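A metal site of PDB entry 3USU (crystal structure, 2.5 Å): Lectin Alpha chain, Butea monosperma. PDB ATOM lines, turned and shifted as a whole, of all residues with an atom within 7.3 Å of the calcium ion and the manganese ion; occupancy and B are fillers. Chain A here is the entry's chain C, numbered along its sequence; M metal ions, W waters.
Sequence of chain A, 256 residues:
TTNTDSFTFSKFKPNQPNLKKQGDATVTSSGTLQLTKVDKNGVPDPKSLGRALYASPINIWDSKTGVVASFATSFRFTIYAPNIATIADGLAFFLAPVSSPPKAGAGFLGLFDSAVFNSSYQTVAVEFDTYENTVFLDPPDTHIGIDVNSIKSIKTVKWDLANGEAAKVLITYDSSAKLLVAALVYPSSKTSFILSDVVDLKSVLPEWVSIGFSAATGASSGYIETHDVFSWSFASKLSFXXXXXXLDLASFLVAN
ND1 of His 143 sits at hydrogen-bond distance from O of Asp 141 (2.9 Å). The backbone carbonyl oxygen (O) of Gly 145 lies within hydrogen-bond range of the backbone NH (N) of Glu 127 (2.9 Å).
Of the 27 residues printed, 4 come within 4 Å of the calcium ion.
Within 4 Å of the manganese ion: Glu 127, Asp 129, Asp 138 and His 143.
Water W4 is bound to the calcium ion (2.1 Å). O of Tyr 131 is bound to the calcium ion (2.4 Å). The calcium ion is bound by water W1 (2.4 Å). The side-chain carboxylate (OD1) of Asp 129 binds the calcium ion, at 2.4 Å. The side-chain amide oxygen (OD1) of Asn 133 binds the calcium ion, at 2.4 Å. OD2 of Asp 129 is bound to the calcium ion, 2.5 Å away. The calcium ion is bound by the side-chain carboxylate (OD2) of Asp 138, at 2.7 Å.
The manganese ion is bound by water W3, at 2.1 Å. OD2 of Asp 129 binds the manganese ion (2.2 Å). OD1 of Asp 138 binds the manganese ion (2.2 Å). NE2 of His 143 binds the manganese ion, 2.3 Å away. The manganese ion is bound by water W2, 2.3 Å away. OE2 of Glu 127 is bound to the manganese ion (2.4 Å).
Water W2 bridges the side-chain carboxylate (OE1) of Glu 127 (2.8 Å) and the backbone carbonyl oxygen (O) of Ile 151 (3.0 Å).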
ATOM      1  N   ASP A  89     -16.490 -15.429  19.973  1.00  0.00           N
ATOM      2  CA  ASP A  89     -16.110 -14.636  18.851  1.00  0.00           C
ATOM      3  C   ASP A  89     -16.804 -13.287  18.750  1.00  0.00           C
ATOM      4  O   ASP A  89     -16.151 -12.306  18.419  1.00  0.00           O
ATOM      5  CB  ASP A  89     -16.197 -15.408  17.546  1.00  0.00           C
ATOM      6  CG  ASP A  89     -14.894 -15.999  17.151  1.00  0.00           C
ATOM      7  OD1 ASP A  89     -14.815 -17.224  17.165  1.00  0.00           O
ATOM      8  OD2 ASP A  89     -13.931 -15.227  16.877  1.00  0.00           O
ATOM      9  N   GLY A  90     -18.108 -13.230  19.011  1.00  0.00           N
ATOM     10  CA  GLY A  90     -18.877 -11.991  18.884  1.00  0.00           C
ATOM     11  C   GLY A  90     -20.332 -12.234  18.561  1.00  0.00           C
ATOM     12  O   GLY A  90     -20.751 -13.361  18.344  1.00  0.00           O
ATOM     13  N   ALA A 106     -17.529 -19.291  14.573  1.00  0.00           N
ATOM     14  CA  ALA A 106     -16.320 -18.680  15.014  1.00  0.00           C
ATOM     15  C   ALA A 106     -16.246 -17.168  14.682  1.00  0.00           C
ATOM     16  O   ALA A 106     -17.162 -16.410  14.962  1.00  0.00           O
ATOM     17  CB  ALA A 106     -15.124 -19.486  14.520  1.00  0.00           C
ATOM     18  N   GLY A 107     -15.169 -16.720  14.061  1.00  0.00           N
ATOM     19  CA  GLY A 107     -15.129 -15.372  13.565  1.00  0.00           C
ATOM     20  C   GLY A 107     -16.088 -14.997  12.437  1.00  0.00           C
ATOM     21  O   GLY A 107     -16.318 -13.785  12.193  1.00  0.00           O
ATOM     22  N   PHE A 108     -16.661 -15.991  11.741  1.00  0.00           N
ATOM     23  CA  PHE A 108     -17.678 -15.690  10.719  1.00  0.00           C
ATOM     24  C   PHE A 108     -19.022 -15.279  11.350  1.00  0.00           C
ATOM     25  O   PHE A 108     -19.914 -14.830  10.627  1.00  0.00           O
ATOM     26  CB  PHE A 108     -17.942 -16.887   9.779  1.00  0.00           C
ATOM     27  CG  PHE A 108     -16.686 -17.528   9.200  1.00  0.00           C
ATOM     28  CD1 PHE A 108     -16.042 -16.987   8.103  1.00  0.00           C
ATOM     29  CD2 PHE A 108     -16.174 -18.686   9.763  1.00  0.00           C
ATOM     30  CE1 PHE A 108     -14.924 -17.578   7.596  1.00  0.00           C
ATOM     31  CE2 PHE A 108     -15.046 -19.279   9.246  1.00  0.00           C
ATOM     32  CZ  PHE A 108     -14.420 -18.715   8.158  1.00  0.00           C
ATOM     33  N   LEU A 109     -19.162 -15.475  12.672  1.00  0.00           N
ATOM     34  CA  LEU A 109     -20.315 -15.004  13.457  1.00  0.00           C
ATOM     35  C   LEU A 109     -21.691 -15.581  13.015  1.00  0.00           C
ATOM     36  O   LEU A 109     -22.742 -15.068  13.405  1.00  0.00           O
ATOM     37  CB  LEU A 109     -20.348 -13.473  13.448  1.00  0.00           C
ATOM     38  CG  LEU A 109     -19.124 -12.733  13.962  1.00  0.00           C
ATOM     39  CD1 LEU A 109     -19.316 -11.236  13.803  1.00  0.00           C
ATOM     40  CD2 LEU A 109     -18.880 -13.080  15.427  1.00  0.00           C
ATOM     41  N   GLU A 127     -22.116  -5.621  13.701  1.00  0.00           N
ATOM     42  CA  GLU A 127     -21.247  -6.601  14.317  1.00  0.00           C
ATOM     43  C   GLU A 127     -20.782  -6.170  15.732  1.00  0.00           C
ATOM     44  O   GLU A 127     -20.466  -4.977  15.963  1.00  0.00           O
ATOM     45  CB  GLU A 127     -20.052  -6.640  13.399  1.00  0.00           C
ATOM     46  CG  GLU A 127     -19.303  -7.934  13.383  1.00  0.00           C
ATOM     47  CD  GLU A 127     -18.062  -7.759  12.570  1.00  0.00           C
ATOM     48  OE1 GLU A 127     -18.066  -8.244  11.434  1.00  0.00           O
ATOM     49  OE2 GLU A 127     -17.095  -7.123  13.047  1.00  0.00           O
ATOM     50  N   PHE A 128     -20.696  -7.110  16.661  1.00  0.00           N
ATOM     51  CA  PHE A 128     -20.058  -6.803  17.926  1.00  0.00           C
ATOM     52  C   PHE A 128     -18.922  -7.794  18.118  1.00  0.00           C
ATOM     53  O   PHE A 128     -19.156  -8.939  18.483  1.00  0.00           O
ATOM     54  CB  PHE A 128     -21.082  -6.823  19.054  1.00  0.00           C
ATOM     55  CG  PHE A 128     -22.151  -5.781  18.877  1.00  0.00           C
ATOM     56  CD1 PHE A 128     -22.020  -4.537  19.448  1.00  0.00           C
ATOM     57  CD2 PHE A 128     -23.251  -6.027  18.035  1.00  0.00           C
ATOM     58  CE1 PHE A 128     -22.975  -3.562  19.237  1.00  0.00           C
ATOM     59  CE2 PHE A 128     -24.205  -5.052  17.804  1.00  0.00           C
ATOM     60  CZ  PHE A 128     -24.068  -3.820  18.415  1.00  0.00           C
ATOM     61  N   ASP A 129     -17.706  -7.363  17.846  1.00  0.00           N
ATOM     62  CA  ASP A 129     -16.643  -8.314  17.513  1.00  0.00           C
ATOM     63  C   ASP A 129     -15.656  -8.421  18.676  1.00  0.00           C
ATOM     64  O   ASP A 129     -15.156  -7.401  19.127  1.00  0.00           O
ATOM     65  CB  ASP A 129     -15.947  -7.937  16.157  1.00  0.00           C
ATOM     66  CG  ASP A 129     -15.082  -9.087  15.599  1.00  0.00           C
ATOM     67  OD1 ASP A 129     -14.632  -9.937  16.431  1.00  0.00           O
ATOM     68  OD2 ASP A 129     -14.876  -9.175  14.329  1.00  0.00           O
ATOM     69  N   THR A 130     -15.391  -9.642  19.152  1.00  0.00           N
ATOM     70  CA  THR A 130     -14.642  -9.816  20.389  1.00  0.00           C
ATOM     71  C   THR A 130     -13.249 -10.455  20.230  1.00  0.00           C
ATOM     72  O   THR A 130     -12.545 -10.689  21.233  1.00  0.00           O
ATOM     73  CB  THR A 130     -15.433 -10.618  21.435  1.00  0.00           C
ATOM     74  OG1 THR A 130     -15.767 -11.914  20.911  1.00  0.00           O
ATOM     75  CG2 THR A 130     -16.704  -9.851  21.894  1.00  0.00           C
ATOM     76  N   TYR A 131     -12.883 -10.750  18.987  1.00  0.00           N
ATOM     77  CA  TYR A 131     -11.637 -11.414  18.678  1.00  0.00           C
ATOM     78  C   TYR A 131     -11.067 -10.848  17.366  1.00  0.00           C
ATOM     79  O   TYR A 131     -11.794 -10.701  16.360  1.00  0.00           O
ATOM     80  CB  TYR A 131     -11.896 -12.921  18.568  1.00  0.00           C
ATOM     81  CG  TYR A 131     -10.714 -13.786  18.152  1.00  0.00           C
ATOM     82  CD1 TYR A 131      -9.772 -14.226  19.079  1.00  0.00           C
ATOM     83  CD2 TYR A 131     -10.572 -14.198  16.815  1.00  0.00           C
ATOM     84  CE1 TYR A 131      -8.716 -15.043  18.686  1.00  0.00           C
ATOM     85  CE2 TYR A 131      -9.522 -14.993  16.412  1.00  0.00           C
ATOM     86  CZ  TYR A 131      -8.590 -15.422  17.348  1.00  0.00           C
ATOM     87  OH  TYR A 131      -7.540 -16.218  16.945  1.00  0.00           O
ATOM     88  N   GLU A 132      -9.774 -10.534  17.359  1.00  0.00           N
ATOM     89  CA  GLU A 132      -9.184 -10.074  16.127  1.00  0.00           C
ATOM     90  C   GLU A 132      -8.913 -11.187  15.092  1.00  0.00           C
ATOM     91  O   GLU A 132      -8.042 -12.048  15.308  1.00  0.00           O
ATOM     92  CB  GLU A 132      -7.934  -9.253  16.403  1.00  0.00           C
ATOM     93  CG  GLU A 132      -7.307  -8.696  15.134  1.00  0.00           C
ATOM     94  CD  GLU A 132      -6.062  -7.915  15.399  1.00  0.00           C
ATOM     95  OE1 GLU A 132      -5.244  -8.306  16.308  1.00  0.00           O
ATOM     96  OE2 GLU A 132      -5.919  -6.912  14.686  1.00  0.00           O
ATOM     97  N   ASN A 133      -9.620 -11.162  13.956  1.00  0.00           N
ATOM     98  CA  ASN A 133      -9.268 -12.043  12.828  1.00  0.00           C
ATOM     99  C   ASN A 133      -8.529 -11.254  11.778  1.00  0.00           C
ATOM    100  O   ASN A 133      -9.158 -10.489  11.005  1.00  0.00           O
ATOM    101  CB  ASN A 133     -10.502 -12.636  12.174  1.00  0.00           C
ATOM    102  CG  ASN A 133     -11.326 -13.502  13.097  1.00  0.00           C
ATOM    103  OD1 ASN A 133     -12.347 -13.067  13.629  1.00  0.00           O
ATOM    104  ND2 ASN A 133     -10.924 -14.747  13.241  1.00  0.00           N
ATOM    105  N   THR A 134      -7.195 -11.421  11.740  1.00  0.00           N
ATOM    106  CA  THR A 134      -6.376 -10.666  10.805  1.00  0.00           C
ATOM    107  C   THR A 134      -6.775 -11.066   9.384  1.00  0.00           C
ATOM    108  O   THR A 134      -6.648 -10.259   8.438  1.00  0.00           O
ATOM    109  CB  THR A 134      -4.832 -10.799  11.071  1.00  0.00           C
ATOM    110  OG1 THR A 134      -4.512 -12.139  11.499  1.00  0.00           O
ATOM    111  CG2 THR A 134      -4.372  -9.846  12.180  1.00  0.00           C
ATOM    112  N   PHE A 136      -9.592 -11.142   8.207  1.00  0.00           N
ATOM    113  CA  PHE A 136     -10.777 -10.362   7.799  1.00  0.00           C
ATOM    114  C   PHE A 136     -10.528  -8.844   7.929  1.00  0.00           C
ATOM    115  O   PHE A 136     -11.487  -8.014   7.927  1.00  0.00           O
ATOM    116  CB  PHE A 136     -12.009 -10.730   8.661  1.00  0.00           C
ATOM    117  CG  PHE A 136     -12.329 -12.221   8.748  1.00  0.00           C
ATOM    118  CD1 PHE A 136     -12.235 -13.064   7.634  1.00  0.00           C
ATOM    119  CD2 PHE A 136     -12.787 -12.762   9.947  1.00  0.00           C
ATOM    120  CE1 PHE A 136     -12.546 -14.425   7.733  1.00  0.00           C
ATOM    121  CE2 PHE A 136     -13.117 -14.120  10.034  1.00  0.00           C
ATOM    122  CZ  PHE A 136     -12.983 -14.959   8.933  1.00  0.00           C
ATOM    123  N   LEU A 137      -9.257  -8.479   8.081  1.00  0.00           N
ATOM    124  CA  LEU A 137      -8.887  -7.104   8.377  1.00  0.00           C
ATOM    125  C   LEU A 137      -9.425  -6.522   9.672  1.00  0.00           C
ATOM    126  O   LEU A 137      -9.624  -5.311   9.751  1.00  0.00           O
ATOM    127  CB  LEU A 137      -9.233  -6.172   7.202  1.00  0.00           C
ATOM    128  CG  LEU A 137      -7.900  -5.772   6.587  1.00  0.00           C
ATOM    129  CD1 LEU A 137      -7.847  -6.096   5.094  1.00  0.00           C
ATOM    130  CD2 LEU A 137      -7.590  -4.307   6.930  1.00  0.00           C
ATOM    131  N   ASP A 138      -9.622  -7.351  10.694  1.00  0.00           N
ATOM    132  CA  ASP A 138     -10.066  -6.813  11.994  1.00  0.00           C
ATOM    133  C   ASP A 138      -9.062  -5.862  12.656  1.00  0.00           C
ATOM    134  O   ASP A 138      -7.928  -6.206  12.824  1.00  0.00           O
ATOM    135  CB  ASP A 138     -10.376  -7.948  12.976  1.00  0.00           C
ATOM    136  CG  ASP A 138     -11.760  -8.557  12.734  1.00  0.00           C
ATOM    137  OD1 ASP A 138     -12.643  -7.820  12.245  1.00  0.00           O
ATOM    138  OD2 ASP A 138     -11.961  -9.777  13.042  1.00  0.00           O
ATOM    139  N   PRO A 139      -9.492  -4.653  13.041  1.00  0.00           N
ATOM    140  CA  PRO A 139      -8.644  -3.844  13.913  1.00  0.00           C
ATOM    141  C   PRO A 139      -8.145  -4.528  15.190  1.00  0.00           C
ATOM    142  O   PRO A 139      -8.767  -5.487  15.714  1.00  0.00           O
ATOM    143  CB  PRO A 139      -9.597  -2.761  14.415  1.00  0.00           C
ATOM    144  CG  PRO A 139     -10.958  -3.293  14.175  1.00  0.00           C
ATOM    145  CD  PRO A 139     -10.811  -4.050  12.885  1.00  0.00           C
ATOM    146  N   ASP A 141      -8.246  -3.850  18.186  1.00  0.00           N
ATOM    147  CA  ASP A 141      -9.131  -3.872  19.353  1.00  0.00           C
ATOM    148  C   ASP A 141     -10.523  -4.469  19.111  1.00  0.00           C
ATOM    149  O   ASP A 141     -10.928  -4.661  17.972  1.00  0.00           O
ATOM    150  CB  ASP A 141      -9.262  -2.468  19.969  1.00  0.00           C
ATOM    151  CG  ASP A 141      -7.982  -1.982  20.594  1.00  0.00           C
ATOM    152  OD1 ASP A 141      -7.530  -2.533  21.639  1.00  0.00           O
ATOM    153  OD2 ASP A 141      -7.391  -1.038  20.038  1.00  0.00           O
ATOM    154  N   HIS A 143     -14.387  -4.333  18.702  1.00  0.00           N
ATOM    155  CA  HIS A 143     -14.936  -3.265  17.866  1.00  0.00           C
ATOM    156  C   HIS A 143     -16.362  -3.522  17.514  1.00  0.00           C
ATOM    157  O   HIS A 143     -16.798  -4.681  17.507  1.00  0.00           O
ATOM    158  CB  HIS A 143     -14.045  -3.092  16.620  1.00  0.00           C
ATOM    159  CG  HIS A 143     -13.948  -4.344  15.773  1.00  0.00           C
ATOM    160  ND1 HIS A 143     -12.981  -5.260  15.945  1.00  0.00           N
ATOM    161  CD2 HIS A 143     -14.769  -4.831  14.766  1.00  0.00           C
ATOM    162  CE1 HIS A 143     -13.161  -6.278  15.073  1.00  0.00           C
ATOM    163  NE2 HIS A 143     -14.254  -6.022  14.356  1.00  0.00           N
ATOM    164  N   ILE A 144     -17.121  -2.465  17.286  1.00  0.00           N
ATOM    165  CA  ILE A 144     -18.348  -2.592  16.497  1.00  0.00           C
ATOM    166  C   ILE A 144     -17.986  -2.325  15.019  1.00  0.00           C
ATOM    167  O   ILE A 144     -17.011  -1.615  14.726  1.00  0.00           O
ATOM    168  CB  ILE A 144     -19.409  -1.573  16.952  1.00  0.00           C
ATOM    169  CG1 ILE A 144     -19.754  -1.792  18.431  1.00  0.00           C
ATOM    170  CG2 ILE A 144     -20.649  -1.616  16.093  1.00  0.00           C
ATOM    171  CD1 ILE A 144     -19.977  -0.478  19.171  1.00  0.00           C
ATOM    172  N   GLY A 145     -18.724  -2.906  14.076  1.00  0.00           N
ATOM    173  CA  GLY A 145     -18.414  -2.694  12.655  1.00  0.00           C
ATOM    174  C   GLY A 145     -19.633  -2.932  11.805  1.00  0.00           C
ATOM    175  O   GLY A 145     -20.499  -3.690  12.175  1.00  0.00           O
ATOM    176  N   ASP A 147     -21.026  -4.585   8.487  1.00  0.00           N
ATOM    177  CA  ASP A 147     -20.700  -5.586   7.487  1.00  0.00           C
ATOM    178  C   ASP A 147     -21.703  -5.568   6.372  1.00  0.00           C
ATOM    179  O   ASP A 147     -22.891  -5.609   6.649  1.00  0.00           O
ATOM    180  CB  ASP A 147     -20.712  -6.971   8.114  1.00  0.00           C
ATOM    181  CG  ASP A 147     -19.789  -7.079   9.313  1.00  0.00           C
ATOM    182  OD1 ASP A 147     -19.056  -6.080   9.558  1.00  0.00           O
ATOM    183  OD2 ASP A 147     -19.816  -8.139   9.993  1.00  0.00           O
ATOM    184  N   ILE A 151     -17.606 -10.382   5.772  1.00  0.00           N
ATOM    185  CA  ILE A 151     -17.153 -10.445   7.162  1.00  0.00           C
ATOM    186  C   ILE A 151     -16.112  -9.340   7.417  1.00  0.00           C
ATOM    187  O   ILE A 151     -15.829  -9.019   8.550  1.00  0.00           O
ATOM    188  CB  ILE A 151     -16.671 -11.888   7.509  1.00  0.00           C
ATOM    189  CG1 ILE A 151     -16.351 -12.053   9.001  1.00  0.00           C
ATOM    190  CG2 ILE A 151     -15.495 -12.290   6.677  1.00  0.00           C
ATOM    191  CD1 ILE A 151     -17.483 -11.660   9.936  1.00  0.00           C
ATOM    192  N   LYS A 152     -15.542  -8.738   6.366  1.00  0.00           N
ATOM    193  CA  LYS A 152     -14.660  -7.578   6.531  1.00  0.00           C
ATOM    194  C   LYS A 152     -15.497  -6.302   6.611  1.00  0.00           C
ATOM    195  O   LYS A 152     -15.985  -5.847   5.603  1.00  0.00           O
ATOM    196  CB  LYS A 152     -13.634  -7.426   5.364  1.00  0.00           C
ATOM    197  CG  LYS A 152     -12.858  -8.696   4.970  1.00  0.00           C
ATOM    198  CD  LYS A 152     -11.514  -8.388   4.275  1.00  0.00           C
ATOM    199  CE  LYS A 152     -10.784  -9.661   3.807  1.00  0.00           C
ATOM    200  NZ  LYS A 152     -11.722 -10.757   3.368  1.00  0.00           N
ATOM    201  N   SER A 153     -15.612  -5.720   7.781  1.00  0.00           N
ATOM    202  CA  SER A 153     -16.369  -4.488   7.936  1.00  0.00           C
ATOM    203  C   SER A 153     -16.014  -3.400   6.926  1.00  0.00           C
ATOM    204  O   SER A 153     -14.869  -3.300   6.507  1.00  0.00           O
ATOM    205  CB  SER A 153     -16.217  -3.971   9.363  1.00  0.00           C
ATOM    206  OG  SER A 153     -16.501  -5.017  10.298  1.00  0.00           O
ATOM    207  N   THR A 156     -15.427   0.428  11.196  1.00  0.00           N
ATOM    208  CA  THR A 156     -15.455  -0.088  12.562  1.00  0.00           C
ATOM    209  C   THR A 156     -15.148   1.072  13.533  1.00  0.00           C
ATOM    210  O   THR A 156     -14.756   2.174  13.117  1.00  0.00           O
ATOM    211  CB  THR A 156     -14.412  -1.208  12.797  1.00  0.00           C
ATOM    212  OG1 THR A 156     -13.163  -0.807  12.247  1.00  0.00           O
ATOM    213  CG2 THR A 156     -14.789  -2.514  12.120  1.00  0.00           C
HETATM  214 CA    CA M   1     -13.451 -11.194  14.740  1.00  0.00          CA
HETATM  215 MN    MN M   2     -14.777  -7.625  12.836  1.00  0.00          MN
HETATM  216  O   HOH W   1     -14.843 -11.397  12.818  1.00  0.00           O
HETATM  217  O   HOH W   2     -15.488  -9.406  11.483  1.00  0.00           O
HETATM  218  O   HOH W   3     -14.794  -5.913  11.668  1.00  0.00           O
HETATM  219  O   HOH W   4     -14.553 -12.824  15.518  1.00  0.00           O
